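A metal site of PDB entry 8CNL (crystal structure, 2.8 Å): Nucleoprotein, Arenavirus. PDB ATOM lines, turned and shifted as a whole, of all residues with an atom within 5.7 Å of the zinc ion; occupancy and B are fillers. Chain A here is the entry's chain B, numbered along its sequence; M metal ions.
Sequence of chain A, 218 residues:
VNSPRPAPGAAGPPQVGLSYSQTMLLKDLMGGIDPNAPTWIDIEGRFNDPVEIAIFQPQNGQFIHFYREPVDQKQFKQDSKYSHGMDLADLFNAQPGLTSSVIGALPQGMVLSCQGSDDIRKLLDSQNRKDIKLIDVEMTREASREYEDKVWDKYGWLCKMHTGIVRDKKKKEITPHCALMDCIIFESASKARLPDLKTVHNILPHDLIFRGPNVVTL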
ATOM      1  N   GLU A  52      -7.906  19.152  -6.816  1.00  0.00           N
ATOM      2  CA  GLU A  52      -8.832  19.098  -5.691  1.00  0.00           C
ATOM      3  C   GLU A  52      -9.401  20.482  -5.430  1.00  0.00           C
ATOM      4  O   GLU A  52      -8.645  21.442  -5.303  1.00  0.00           O
ATOM      5  CB  GLU A  52      -8.151  18.567  -4.444  1.00  0.00           C
ATOM      6  CG  GLU A  52      -8.992  18.583  -3.178  1.00  0.00           C
ATOM      7  CD  GLU A  52      -8.134  18.342  -1.913  1.00  0.00           C
ATOM      8  OE1 GLU A  52      -7.153  19.097  -1.726  1.00  0.00           O
ATOM      9  OE2 GLU A  52      -8.424  17.401  -1.130  1.00  0.00           O
ATOM     10  N   HIS A  65     -16.625  19.682  -2.004  1.00  0.00           N
ATOM     11  CA  HIS A  65     -15.236  19.218  -1.969  1.00  0.00           C
ATOM     12  C   HIS A  65     -15.091  17.995  -2.855  1.00  0.00           C
ATOM     13  O   HIS A  65     -15.729  16.978  -2.590  1.00  0.00           O
ATOM     14  CB  HIS A  65     -14.831  18.932  -0.492  1.00  0.00           C
ATOM     15  CG  HIS A  65     -13.545  18.180  -0.319  1.00  0.00           C
ATOM     16  ND1 HIS A  65     -12.335  18.631  -0.795  1.00  0.00           N
ATOM     17  CD2 HIS A  65     -13.282  17.010   0.318  1.00  0.00           C
ATOM     18  CE1 HIS A  65     -11.389  17.764  -0.484  1.00  0.00           C
ATOM     19  NE2 HIS A  65     -11.923  16.770   0.184  1.00  0.00           N
ATOM     20  N   TYR A  67     -12.488  16.036  -6.344  1.00  0.00           N
ATOM     21  CA  TYR A  67     -11.173  15.786  -6.903  1.00  0.00           C
ATOM     22  C   TYR A  67     -11.271  15.726  -8.417  1.00  0.00           C
ATOM     23  O   TYR A  67     -12.360  15.629  -9.003  1.00  0.00           O
ATOM     24  CB  TYR A  67     -10.604  14.485  -6.370  1.00  0.00           C
ATOM     25  CG  TYR A  67     -10.722  14.412  -4.881  1.00  0.00           C
ATOM     26  CD1 TYR A  67      -9.933  15.214  -4.075  1.00  0.00           C
ATOM     27  CD2 TYR A  67     -11.624  13.555  -4.264  1.00  0.00           C
ATOM     28  CE1 TYR A  67     -10.037  15.163  -2.691  1.00  0.00           C
ATOM     29  CE2 TYR A  67     -11.728  13.490  -2.880  1.00  0.00           C
ATOM     30  CZ  TYR A  67     -10.932  14.311  -2.097  1.00  0.00           C
ATOM     31  OH  TYR A  67     -10.988  14.309  -0.722  1.00  0.00           O
ATOM     32  N   MET A  86      -0.632  14.037  -2.938  1.00  0.00           N
ATOM     33  CA  MET A  86      -1.688  13.135  -3.347  1.00  0.00           C
ATOM     34  C   MET A  86      -1.116  12.001  -4.183  1.00  0.00           C
ATOM     35  O   MET A  86       0.035  12.036  -4.635  1.00  0.00           O
ATOM     36  CB  MET A  86      -2.744  13.890  -4.138  1.00  0.00           C
ATOM     37  CG  MET A  86      -3.363  15.048  -3.386  1.00  0.00           C
ATOM     38  SD  MET A  86      -4.877  15.546  -4.186  1.00  0.00           S
ATOM     39  CE  MET A  86      -5.434  16.883  -3.168  1.00  0.00           C
ATOM     40  N   TRP A 152      -6.344  20.222  11.336  1.00  0.00           N
ATOM     41  CA  TRP A 152      -6.117  18.850  10.826  1.00  0.00           C
ATOM     42  C   TRP A 152      -6.547  17.812  11.854  1.00  0.00           C
ATOM     43  O   TRP A 152      -6.650  16.637  11.487  1.00  0.00           O
ATOM     44  CB  TRP A 152      -4.644  18.679  10.446  1.00  0.00           C
ATOM     45  CG  TRP A 152      -4.274  19.000   9.028  1.00  0.00           C
ATOM     46  CD1 TRP A 152      -3.617  20.113   8.591  1.00  0.00           C
ATOM     47  CD2 TRP A 152      -4.482  18.170   7.873  1.00  0.00           C
ATOM     48  NE1 TRP A 152      -3.423  20.044   7.232  1.00  0.00           N
ATOM     49  CE2 TRP A 152      -3.934  18.869   6.776  1.00  0.00           C
ATOM     50  CE3 TRP A 152      -5.080  16.933   7.661  1.00  0.00           C
ATOM     51  CZ2 TRP A 152      -3.981  18.353   5.477  1.00  0.00           C
ATOM     52  CZ3 TRP A 152      -5.124  16.425   6.374  1.00  0.00           C
ATOM     53  CH2 TRP A 152      -4.576  17.133   5.305  1.00  0.00           C
ATOM     54  N   CYS A 159     -10.873  14.489   4.842  1.00  0.00           N
ATOM     55  CA  CYS A 159     -10.069  14.214   3.628  1.00  0.00           C
ATOM     56  C   CYS A 159      -8.873  13.327   4.008  1.00  0.00           C
ATOM     57  O   CYS A 159      -7.935  13.840   4.636  1.00  0.00           O
ATOM     58  CB  CYS A 159      -9.600  15.507   2.974  1.00  0.00           C
ATOM     59  SG  CYS A 159      -8.809  15.336   1.356  1.00  0.00           S
ATOM     60  N   MET A 161      -6.949  11.905   1.762  1.00  0.00           N
ATOM     61  CA  MET A 161      -6.393  11.803   0.412  1.00  0.00           C
ATOM     62  C   MET A 161      -4.924  12.180   0.307  1.00  0.00           C
ATOM     63  O   MET A 161      -4.365  12.114  -0.782  1.00  0.00           O
ATOM     64  CB  MET A 161      -7.188  12.685  -0.551  1.00  0.00           C
ATOM     65  CG  MET A 161      -8.534  12.110  -0.896  1.00  0.00           C
ATOM     66  SD  MET A 161      -8.415  10.610  -1.903  1.00  0.00           S
ATOM     67  CE  MET A 161      -7.999  11.296  -3.506  1.00  0.00           C
ATOM     68  N   HIS A 162      -4.331  12.661   1.399  1.00  0.00           N
ATOM     69  CA  HIS A 162      -2.927  13.128   1.362  1.00  0.00           C
ATOM     70  C   HIS A 162      -2.051  12.056   2.009  1.00  0.00           C
ATOM     71  O   HIS A 162      -1.676  12.247   3.172  1.00  0.00           O
ATOM     72  CB  HIS A 162      -2.864  14.512   2.015  1.00  0.00           C
ATOM     73  CG  HIS A 162      -3.918  15.422   1.465  1.00  0.00           C
ATOM     74  ND1 HIS A 162      -3.733  16.123   0.303  1.00  0.00           N
ATOM     75  CD2 HIS A 162      -5.169  15.698   1.880  1.00  0.00           C
ATOM     76  CE1 HIS A 162      -4.814  16.817   0.043  1.00  0.00           C
ATOM     77  NE2 HIS A 162      -5.716  16.566   0.973  1.00  0.00           N
ATOM     78  N   HIS A 177      -0.989  20.187   2.122  1.00  0.00           N
ATOM     79  CA  HIS A 177      -2.102  21.164   1.958  1.00  0.00           C
ATOM     80  C   HIS A 177      -3.333  20.420   1.422  1.00  0.00           C
ATOM     81  O   HIS A 177      -3.146  19.551   0.549  1.00  0.00           O
ATOM     82  CB  HIS A 177      -1.635  22.301   1.063  1.00  0.00           C
ATOM     83  CG  HIS A 177      -0.643  23.184   1.733  1.00  0.00           C
ATOM     84  ND1 HIS A 177      -1.003  24.097   2.704  1.00  0.00           N
ATOM     85  CD2 HIS A 177       0.701  23.285   1.600  1.00  0.00           C
ATOM     86  CE1 HIS A 177       0.065  24.731   3.125  1.00  0.00           C
ATOM     87  NE2 HIS A 177       1.119  24.252   2.476  1.00  0.00           N
ATOM     88  N   CYS A 178      -4.529  20.776   1.892  1.00  0.00           N
ATOM     89  CA  CYS A 178      -5.714  19.950   1.530  1.00  0.00           C
ATOM     90  C   CYS A 178      -6.859  20.721   0.879  1.00  0.00           C
ATOM     91  O   CYS A 178      -7.853  20.075   0.613  1.00  0.00           O
ATOM     92  CB  CYS A 178      -6.247  19.296   2.802  1.00  0.00           C
ATOM     93  SG  CYS A 178      -7.774  18.332   2.655  1.00  0.00           S
ATOM     94  N   ALA A 179      -6.757  22.025   0.666  1.00  0.00           N
ATOM     95  CA  ALA A 179      -7.842  22.826   0.067  1.00  0.00           C
ATOM     96  C   ALA A 179      -9.044  22.928   1.012  1.00  0.00           C
ATOM     97  O   ALA A 179      -9.464  24.048   1.285  1.00  0.00           O
ATOM     98  CB  ALA A 179      -8.249  22.305  -1.285  1.00  0.00           C
ATOM     99  N   LEU A 180      -9.612  21.800   1.456  1.00  0.00           N
ATOM    100  CA  LEU A 180     -10.706  21.846   2.447  1.00  0.00           C
ATOM    101  C   LEU A 180     -10.085  22.256   3.763  1.00  0.00           C
ATOM    102  O   LEU A 180     -10.579  23.206   4.376  1.00  0.00           O
ATOM    103  CB  LEU A 180     -11.351  20.466   2.558  1.00  0.00           C
ATOM    104  CG  LEU A 180     -12.402  20.306   3.661  1.00  0.00           C
ATOM    105  CD1 LEU A 180     -13.517  21.340   3.511  1.00  0.00           C
ATOM    106  CD2 LEU A 180     -12.969  18.910   3.643  1.00  0.00           C
HETATM  107 ZN    ZN M   1      -7.488  17.161   0.670  1.00  0.00          ZN
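The backbone carbonyl oxygen of His 177 sits close to a ring nitrogen (ND1) of His 162 (3.5 Å). SG of Cys 159 lies close to OH of Tyr 67 (3.2 Å). SG of Cys 159 lies close to NE2 of His 65.
The zinc ion is bound by NE2 of His 162. OE2 of Glu 52 is bound to the zinc ion (2.0 Å). SG of Cys 178 is bound to the zinc ion (2.3 Å). The side-chain sulfur (SG) of Cys 159 binds the zinc ion (2.4 Å).
Of the 12 residues printed, 4 come within 4 Å of the zinc ion.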
